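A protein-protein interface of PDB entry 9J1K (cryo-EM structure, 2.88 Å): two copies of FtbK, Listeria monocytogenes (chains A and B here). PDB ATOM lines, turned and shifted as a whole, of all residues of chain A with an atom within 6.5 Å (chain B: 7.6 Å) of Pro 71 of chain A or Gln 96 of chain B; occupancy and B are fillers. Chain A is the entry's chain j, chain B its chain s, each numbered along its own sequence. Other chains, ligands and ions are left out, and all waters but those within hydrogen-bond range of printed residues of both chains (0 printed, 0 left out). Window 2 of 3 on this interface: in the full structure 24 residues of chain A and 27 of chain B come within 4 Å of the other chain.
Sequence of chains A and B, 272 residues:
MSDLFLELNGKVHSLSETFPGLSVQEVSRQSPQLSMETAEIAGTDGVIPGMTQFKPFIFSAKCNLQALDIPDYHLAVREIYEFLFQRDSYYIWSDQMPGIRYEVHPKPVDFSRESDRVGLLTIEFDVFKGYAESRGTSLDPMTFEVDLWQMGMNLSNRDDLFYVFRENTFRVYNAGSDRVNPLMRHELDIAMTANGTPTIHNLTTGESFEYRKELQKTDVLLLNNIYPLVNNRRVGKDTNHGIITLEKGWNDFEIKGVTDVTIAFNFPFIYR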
ATOM      1  N   ASP A  69     -17.419   0.401 -21.416  1.00  0.00           N
ATOM      2  CA  ASP A  69     -16.214  -0.411 -21.301  1.00  0.00           C
ATOM      3  C   ASP A  69     -16.596  -1.877 -21.473  1.00  0.00           C
ATOM      4  O   ASP A  69     -17.773  -2.222 -21.608  1.00  0.00           O
ATOM      5  CB  ASP A  69     -15.509  -0.166 -19.964  1.00  0.00           C
ATOM      6  CG  ASP A  69     -16.477  -0.055 -18.808  1.00  0.00           C
ATOM      7  OD1 ASP A  69     -17.052   1.035 -18.616  1.00  0.00           O
ATOM      8  OD2 ASP A  69     -16.663  -1.059 -18.088  1.00  0.00           O
ATOM      9  N   ILE A  70     -15.576  -2.739 -21.470  1.00  0.00           N
ATOM     10  CA  ILE A  70     -15.803  -4.161 -21.742  1.00  0.00           C
ATOM     11  C   ILE A  70     -16.721  -4.815 -20.714  1.00  0.00           C
ATOM     12  O   ILE A  70     -17.663  -5.518 -21.121  1.00  0.00           O
ATOM     13  CB  ILE A  70     -14.456  -4.891 -21.879  1.00  0.00           C
ATOM     14  CG1 ILE A  70     -13.545  -4.149 -22.858  1.00  0.00           C
ATOM     15  CG2 ILE A  70     -14.670  -6.324 -22.330  1.00  0.00           C
ATOM     16  CD1 ILE A  70     -12.401  -3.420 -22.193  1.00  0.00           C
ATOM     17  N   PRO A  71     -16.509  -4.664 -19.399  1.00  0.00           N
ATOM     18  CA  PRO A  71     -17.481  -5.241 -18.455  1.00  0.00           C
ATOM     19  C   PRO A  71     -18.881  -4.696 -18.654  1.00  0.00           C
ATOM     20  O   PRO A  71     -19.861  -5.447 -18.560  1.00  0.00           O
ATOM     21  CB  PRO A  71     -16.907  -4.862 -17.082  1.00  0.00           C
ATOM     22  CG  PRO A  71     -15.465  -4.623 -17.327  1.00  0.00           C
ATOM     23  CD  PRO A  71     -15.392  -4.017 -18.687  1.00  0.00           C
ATOM     24  N   ASP A  72     -18.996  -3.401 -18.951  1.00  0.00           N
ATOM     25  CA  ASP A  72     -20.299  -2.826 -19.255  1.00  0.00           C
ATOM     26  C   ASP A  72     -20.886  -3.448 -20.514  1.00  0.00           C
ATOM     27  O   ASP A  72     -22.096  -3.683 -20.589  1.00  0.00           O
ATOM     28  CB  ASP A  72     -20.185  -1.311 -19.407  1.00  0.00           C
ATOM     29  CG  ASP A  72     -21.529  -0.646 -19.619  1.00  0.00           C
ATOM     30  OD1 ASP A  72     -22.547  -1.198 -19.152  1.00  0.00           O
ATOM     31  OD2 ASP A  72     -21.570   0.427 -20.255  1.00  0.00           O
ATOM     32  N   TYR A  73     -20.044  -3.722 -21.512  1.00  0.00           N
ATOM     33  CA  TYR A  73     -20.528  -4.351 -22.736  1.00  0.00           C
ATOM     34  C   TYR A  73     -21.093  -5.736 -22.456  1.00  0.00           C
ATOM     35  O   TYR A  73     -22.181  -6.085 -22.931  1.00  0.00           O
ATOM     36  CB  TYR A  73     -19.398  -4.425 -23.765  1.00  0.00           C
ATOM     37  CG  TYR A  73     -19.672  -5.365 -24.916  1.00  0.00           C
ATOM     38  CD1 TYR A  73     -20.435  -4.960 -26.001  1.00  0.00           C
ATOM     39  CD2 TYR A  73     -19.157  -6.654 -24.923  1.00  0.00           C
ATOM     40  CE1 TYR A  73     -20.685  -5.815 -27.055  1.00  0.00           C
ATOM     41  CE2 TYR A  73     -19.402  -7.515 -25.971  1.00  0.00           C
ATOM     42  CZ  TYR A  73     -20.166  -7.091 -27.036  1.00  0.00           C
ATOM     43  OH  TYR A  73     -20.410  -7.948 -28.083  1.00  0.00           O
ATOM     44  N   HIS A  74     -20.367  -6.542 -21.678  1.00  0.00           N
ATOM     45  CA  HIS A  74     -20.851  -7.882 -21.364  1.00  0.00           C
ATOM     46  C   HIS A  74     -22.129  -7.828 -20.536  1.00  0.00           C
ATOM     47  O   HIS A  74     -23.068  -8.600 -20.777  1.00  0.00           O
ATOM     48  CB  HIS A  74     -19.766  -8.675 -20.637  1.00  0.00           C
ATOM     49  CG  HIS A  74     -18.674  -9.160 -21.537  1.00  0.00           C
ATOM     50  ND1 HIS A  74     -17.409  -8.613 -21.536  1.00  0.00           N
ATOM     51  CD2 HIS A  74     -18.658 -10.141 -22.470  1.00  0.00           C
ATOM     52  CE1 HIS A  74     -16.661  -9.236 -22.429  1.00  0.00           C
ATOM     53  NE2 HIS A  74     -17.395 -10.168 -23.008  1.00  0.00           N
ATOM     54  N   LEU A  75     -22.187  -6.918 -19.562  1.00  0.00           N
ATOM     55  CA  LEU A  75     -23.393  -6.784 -18.752  1.00  0.00           C
ATOM     56  C   LEU A  75     -24.582  -6.358 -19.603  1.00  0.00           C
ATOM     57  O   LEU A  75     -25.694  -6.869 -19.428  1.00  0.00           O
ATOM     58  CB  LEU A  75     -23.154  -5.786 -17.621  1.00  0.00           C
ATOM     59  CG  LEU A  75     -24.386  -5.393 -16.807  1.00  0.00           C
ATOM     60  CD1 LEU A  75     -24.856  -6.564 -15.963  1.00  0.00           C
ATOM     61  CD2 LEU A  75     -24.089  -4.185 -15.938  1.00  0.00           C
ATOM     62  N   ALA A  76     -24.366  -5.424 -20.531  1.00  0.00           N
ATOM     63  CA  ALA A  76     -25.443  -4.982 -21.407  1.00  0.00           C
ATOM     64  C   ALA A  76     -25.912  -6.108 -22.315  1.00  0.00           C
ATOM     65  O   ALA A  76     -27.114  -6.257 -22.556  1.00  0.00           O
ATOM     66  CB  ALA A  76     -24.989  -3.780 -22.234  1.00  0.00           C
ATOM     67  N   ARG A 113     -19.527  -8.601 -32.468  1.00  0.00           N
ATOM     68  CA  ARG A 113     -18.603  -7.695 -31.796  1.00  0.00           C
ATOM     69  C   ARG A 113     -17.651  -7.089 -32.819  1.00  0.00           C
ATOM     70  O   ARG A 113     -16.834  -7.798 -33.415  1.00  0.00           O
ATOM     71  CB  ARG A 113     -17.836  -8.439 -30.709  1.00  0.00           C
ATOM     72  CG  ARG A 113     -16.901  -7.560 -29.904  1.00  0.00           C
ATOM     73  CD  ARG A 113     -16.863  -7.989 -28.451  1.00  0.00           C
ATOM     74  NE  ARG A 113     -16.381  -6.921 -27.583  1.00  0.00           N
ATOM     75  CZ  ARG A 113     -15.816  -7.117 -26.401  1.00  0.00           C
ATOM     76  NH1 ARG A 113     -15.643  -8.333 -25.911  1.00  0.00           N
ATOM     77  NH2 ARG A 113     -15.411  -6.066 -25.694  1.00  0.00           N
ATOM     78  N   MET B   1      -6.923  -6.941 -20.344  1.00  0.00           N
ATOM     79  CA  MET B   1      -6.615  -8.367 -20.362  1.00  0.00           C
ATOM     80  C   MET B   1      -7.858  -9.185 -20.029  1.00  0.00           C
ATOM     81  O   MET B   1      -8.865  -8.643 -19.572  1.00  0.00           O
ATOM     82  CB  MET B   1      -5.455  -8.669 -19.396  1.00  0.00           C
ATOM     83  CG  MET B   1      -5.799  -8.833 -17.905  1.00  0.00           C
ATOM     84  SD  MET B   1      -6.637 -10.352 -17.397  1.00  0.00           S
ATOM     85  CE  MET B   1      -7.705  -9.730 -16.100  1.00  0.00           C
ATOM     86  N   SER B   2      -7.780 -10.493 -20.258  1.00  0.00           N
ATOM     87  CA  SER B   2      -8.909 -11.378 -20.022  1.00  0.00           C
ATOM     88  C   SER B   2      -8.392 -12.739 -19.586  1.00  0.00           C
ATOM     89  O   SER B   2      -7.235 -13.094 -19.826  1.00  0.00           O
ATOM     90  CB  SER B   2      -9.787 -11.514 -21.272  1.00  0.00           C
ATOM     91  OG  SER B   2      -9.049 -11.211 -22.443  1.00  0.00           O
ATOM     92  N   ASP B   3      -9.269 -13.501 -18.938  1.00  0.00           N
ATOM     93  CA  ASP B   3      -8.922 -14.837 -18.480  1.00  0.00           C
ATOM     94  C   ASP B   3     -10.196 -15.657 -18.357  1.00  0.00           C
ATOM     95  O   ASP B   3     -11.306 -15.119 -18.344  1.00  0.00           O
ATOM     96  CB  ASP B   3      -8.172 -14.799 -17.144  1.00  0.00           C
ATOM     97  CG  ASP B   3      -7.225 -15.967 -16.977  1.00  0.00           C
ATOM     98  OD1 ASP B   3      -7.257 -16.884 -17.824  1.00  0.00           O
ATOM     99  OD2 ASP B   3      -6.448 -15.970 -16.000  1.00  0.00           O
ATOM    100  N   LEU B   4     -10.019 -16.973 -18.283  1.00  0.00           N
ATOM    101  CA  LEU B   4     -11.125 -17.907 -18.118  1.00  0.00           C
ATOM    102  C   LEU B   4     -10.826 -18.799 -16.924  1.00  0.00           C
ATOM    103  O   LEU B   4      -9.774 -19.443 -16.880  1.00  0.00           O
ATOM    104  CB  LEU B   4     -11.330 -18.746 -19.383  1.00  0.00           C
ATOM    105  CG  LEU B   4     -12.593 -19.604 -19.435  1.00  0.00           C
ATOM    106  CD1 LEU B   4     -13.766 -18.791 -19.948  1.00  0.00           C
ATOM    107  CD2 LEU B   4     -12.366 -20.825 -20.306  1.00  0.00           C
ATOM    108  N   PHE B   5     -11.744 -18.834 -15.965  1.00  0.00           N
ATOM    109  CA  PHE B   5     -11.591 -19.644 -14.765  1.00  0.00           C
ATOM    110  C   PHE B   5     -12.470 -20.881 -14.876  1.00  0.00           C
ATOM    111  O   PHE B   5     -13.657 -20.777 -15.206  1.00  0.00           O
ATOM    112  CB  PHE B   5     -11.958 -18.846 -13.515  1.00  0.00           C
ATOM    113  CG  PHE B   5     -10.990 -17.747 -13.193  1.00  0.00           C
ATOM    114  CD1 PHE B   5     -11.117 -16.502 -13.781  1.00  0.00           C
ATOM    115  CD2 PHE B   5      -9.956 -17.959 -12.300  1.00  0.00           C
ATOM    116  CE1 PHE B   5     -10.228 -15.490 -13.486  1.00  0.00           C
ATOM    117  CE2 PHE B   5      -9.064 -16.951 -12.001  1.00  0.00           C
ATOM    118  CZ  PHE B   5      -9.201 -15.715 -12.595  1.00  0.00           C
ATOM    119  N   VAL B  24      -5.971 -15.945 -23.291  1.00  0.00           N
ATOM    120  CA  VAL B  24      -7.336 -15.798 -23.784  1.00  0.00           C
ATOM    121  C   VAL B  24      -7.481 -14.426 -24.425  1.00  0.00           C
ATOM    122  O   VAL B  24      -7.235 -13.400 -23.784  1.00  0.00           O
ATOM    123  CB  VAL B  24      -8.357 -15.990 -22.655  1.00  0.00           C
ATOM    124  CG1 VAL B  24      -9.748 -15.615 -23.134  1.00  0.00           C
ATOM    125  CG2 VAL B  24      -8.329 -17.423 -22.156  1.00  0.00           C
ATOM    126  N   VAL B  27     -13.827 -13.404 -25.117  1.00  0.00           N
ATOM    127  CA  VAL B  27     -14.854 -14.286 -24.580  1.00  0.00           C
ATOM    128  C   VAL B  27     -16.215 -13.779 -25.037  1.00  0.00           C
ATOM    129  O   VAL B  27     -16.458 -12.567 -25.059  1.00  0.00           O
ATOM    130  CB  VAL B  27     -14.770 -14.370 -23.039  1.00  0.00           C
ATOM    131  CG1 VAL B  27     -16.138 -14.188 -22.397  1.00  0.00           C
ATOM    132  CG2 VAL B  27     -14.150 -15.689 -22.616  1.00  0.00           C
ATOM    133  N   TRP B  93     -16.208 -19.484 -15.848  1.00  0.00           N
ATOM    134  CA  TRP B  93     -16.600 -18.079 -15.826  1.00  0.00           C
ATOM    135  C   TRP B  93     -15.424 -17.239 -16.308  1.00  0.00           C
ATOM    136  O   TRP B  93     -14.349 -17.757 -16.615  1.00  0.00           O
ATOM    137  CB  TRP B  93     -17.079 -17.647 -14.435  1.00  0.00           C
ATOM    138  CG  TRP B  93     -16.038 -17.696 -13.364  1.00  0.00           C
ATOM    139  CD1 TRP B  93     -15.167 -16.704 -13.024  1.00  0.00           C
ATOM    140  CD2 TRP B  93     -15.776 -18.784 -12.471  1.00  0.00           C
ATOM    141  NE1 TRP B  93     -14.371 -17.110 -11.982  1.00  0.00           N
ATOM    142  CE2 TRP B  93     -14.725 -18.383 -11.624  1.00  0.00           C
ATOM    143  CE3 TRP B  93     -16.322 -20.059 -12.310  1.00  0.00           C
ATOM    144  CZ2 TRP B  93     -14.209 -19.213 -10.633  1.00  0.00           C
ATOM    145  CZ3 TRP B  93     -15.810 -20.880 -11.325  1.00  0.00           C
ATOM    146  CH2 TRP B  93     -14.765 -20.455 -10.498  1.00  0.00           C
ATOM    147  N   SER B  94     -15.643 -15.929 -16.381  1.00  0.00           N
ATOM    148  CA  SER B  94     -14.652 -14.997 -16.896  1.00  0.00           C
ATOM    149  C   SER B  94     -14.539 -13.796 -15.967  1.00  0.00           C
ATOM    150  O   SER B  94     -15.455 -13.485 -15.203  1.00  0.00           O
ATOM    151  CB  SER B  94     -15.003 -14.528 -18.313  1.00  0.00           C
ATOM    152  OG  SER B  94     -16.087 -13.617 -18.291  1.00  0.00           O
ATOM    153  N   ASP B  95     -13.390 -13.119 -16.048  1.00  0.00           N
ATOM    154  CA  ASP B  95     -13.151 -11.957 -15.198  1.00  0.00           C
ATOM    155  C   ASP B  95     -14.049 -10.785 -15.571  1.00  0.00           C
ATOM    156  O   ASP B  95     -14.310  -9.918 -14.730  1.00  0.00           O
ATOM    157  CB  ASP B  95     -11.685 -11.539 -15.280  1.00  0.00           C
ATOM    158  CG  ASP B  95     -10.847 -12.519 -16.070  1.00  0.00           C
ATOM    159  OD1 ASP B  95     -11.104 -13.735 -15.964  1.00  0.00           O
ATOM    160  OD2 ASP B  95      -9.938 -12.074 -16.799  1.00  0.00           O
ATOM    161  N   GLN B  96     -14.513 -10.730 -16.820  1.00  0.00           N
ATOM    162  CA  GLN B  96     -15.376  -9.629 -17.236  1.00  0.00           C
ATOM    163  C   GLN B  96     -16.703  -9.651 -16.489  1.00  0.00           C
ATOM    164  O   GLN B  96     -17.223  -8.597 -16.105  1.00  0.00           O
ATOM    165  CB  GLN B  96     -15.601  -9.683 -18.746  1.00  0.00           C
ATOM    166  CG  GLN B  96     -14.679  -8.769 -19.537  1.00  0.00           C
ATOM    167  CD  GLN B  96     -13.215  -8.979 -19.206  1.00  0.00           C
ATOM    168  OE1 GLN B  96     -12.773 -10.103 -18.967  1.00  0.00           O
ATOM    169  NE2 GLN B  96     -12.451  -7.893 -19.186  1.00  0.00           N
ATOM    170  N   MET B  97     -17.265 -10.837 -16.276  1.00  0.00           N
ATOM    171  CA  MET B  97     -18.485 -11.016 -15.490  1.00  0.00           C
ATOM    172  C   MET B  97     -18.231 -12.102 -14.454  1.00  0.00           C
ATOM    173  O   MET B  97     -18.729 -13.227 -14.574  1.00  0.00           O
ATOM    174  CB  MET B  97     -19.673 -11.367 -16.385  1.00  0.00           C
ATOM    175  CG  MET B  97     -20.950 -10.628 -16.033  1.00  0.00           C
ATOM    176  SD  MET B  97     -21.967 -10.280 -17.478  1.00  0.00           S
ATOM    177  CE  MET B  97     -22.089 -11.912 -18.201  1.00  0.00           C
ATOM    178  N   PRO B  98     -17.445 -11.794 -13.418  1.00  0.00           N
ATOM    179  CA  PRO B  98     -17.047 -12.839 -12.463  1.00  0.00           C
ATOM    180  C   PRO B  98     -18.195 -13.407 -11.651  1.00  0.00           C
ATOM    181  O   PRO B  98     -18.050 -14.505 -11.103  1.00  0.00           O
ATOM    182  CB  PRO B  98     -16.035 -12.120 -11.564  1.00  0.00           C
ATOM    183  CG  PRO B  98     -16.446 -10.692 -11.621  1.00  0.00           C
ATOM    184  CD  PRO B  98     -16.977 -10.460 -13.008  1.00  0.00           C
ATOM    185  N   GLY B  99     -19.321 -12.712 -11.556  1.00  0.00           N
ATOM    186  CA  GLY B  99     -20.397 -13.158 -10.697  1.00  0.00           C
ATOM    187  C   GLY B  99     -21.321 -14.203 -11.272  1.00  0.00           C
ATOM    188  O   GLY B  99     -22.269 -14.609 -10.594  1.00  0.00           O
ATOM    189  N   ASP B 147     -19.649 -10.063  -7.211  1.00  0.00           N
ATOM    190  CA  ASP B 147     -20.344  -9.011  -7.950  1.00  0.00           C
ATOM    191  C   ASP B 147     -21.649  -9.547  -8.518  1.00  0.00           C
ATOM    192  O   ASP B 147     -21.730 -10.722  -8.890  1.00  0.00           O
ATOM    193  CB  ASP B 147     -19.478  -8.453  -9.084  1.00  0.00           C
ATOM    194  CG  ASP B 147     -18.945  -7.067  -8.779  1.00  0.00           C
ATOM    195  OD1 ASP B 147     -19.598  -6.335  -8.006  1.00  0.00           O
ATOM    196  OD2 ASP B 147     -17.872  -6.711  -9.309  1.00  0.00           O
ATOM    197  N   TRP B 149     -24.786  -7.478 -10.892  1.00  0.00           N
ATOM    198  CA  TRP B 149     -25.445  -6.260 -11.343  1.00  0.00           C
ATOM    199  C   TRP B 149     -26.796  -6.597 -11.955  1.00  0.00           C
ATOM    200  O   TRP B 149     -26.888  -7.464 -12.830  1.00  0.00           O
ATOM    201  CB  TRP B 149     -24.577  -5.511 -12.355  1.00  0.00           C
ATOM    202  CG  TRP B 149     -23.345  -4.925 -11.753  1.00  0.00           C
ATOM    203  CD1 TRP B 149     -22.159  -5.558 -11.537  1.00  0.00           C
ATOM    204  CD2 TRP B 149     -23.179  -3.585 -11.278  1.00  0.00           C
ATOM    205  NE1 TRP B 149     -21.260  -4.694 -10.960  1.00  0.00           N
ATOM    206  CE2 TRP B 149     -21.864  -3.476 -10.791  1.00  0.00           C
ATOM    207  CE3 TRP B 149     -24.016  -2.468 -11.220  1.00  0.00           C
ATOM    208  CZ2 TRP B 149     -21.365  -2.293 -10.252  1.00  0.00           C
ATOM    209  CZ3 TRP B 149     -23.520  -1.295 -10.686  1.00  0.00           C
ATOM    210  CH2 TRP B 149     -22.206  -1.217 -10.208  1.00  0.00           C
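No position is printed for both chains.
Of the 7 pairs that touch across the chains among the printed residues, none has its exchanged pair printed and touching as well.
Hydrophobic or aromatic side chains of chain B that line the printed part of chain A: Met 97 and Trp 149.
Among the printed residues, no Asp or Glu carboxylate lies within 4 Å of a Lys or Arg side-chain nitrogen of the other chain.
NE2 of His 74 of chain A sits at hydrogen-bond distance from O of Val 27 of chain B (3.3 Å).
Among the printed residues, merely in contact across the chains: His 74 of chain A with Gln 96 of chain B, Ile 70 of chain A with Gln 96 of chain B, Leu 75 of chain A with Trp 149 of chain B, His 74 of chain A with Met 97 of chain B, Pro 71 of chain A with Gln 96 of chain B and Leu 75 of chain A with Met 97 of chain B.
ND1 of His 74 of chain A sits at hydrogen-bond distance from O of Ile 70 of chain A, 3.1 Å away.
Of chain B, only Gln 96 (3.9 Å) comes within 4 Å of Pro 71 of chain A.
Gln 96 of chain B touches three residues of chain A.
Of the printed residues of chain B, Ile 70 of chain A touches Gln 96 (3.7 Å).
Of the printed residues of chain A, Trp 149 of chain B touches Leu 75 (3.8 Å).
Asp 3 of chain B touches none of the printed residues of chain A.
The nearest residue of chain B that does not touch Pro 71 of chain A is Met 97 of chain B (5.4 Å).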
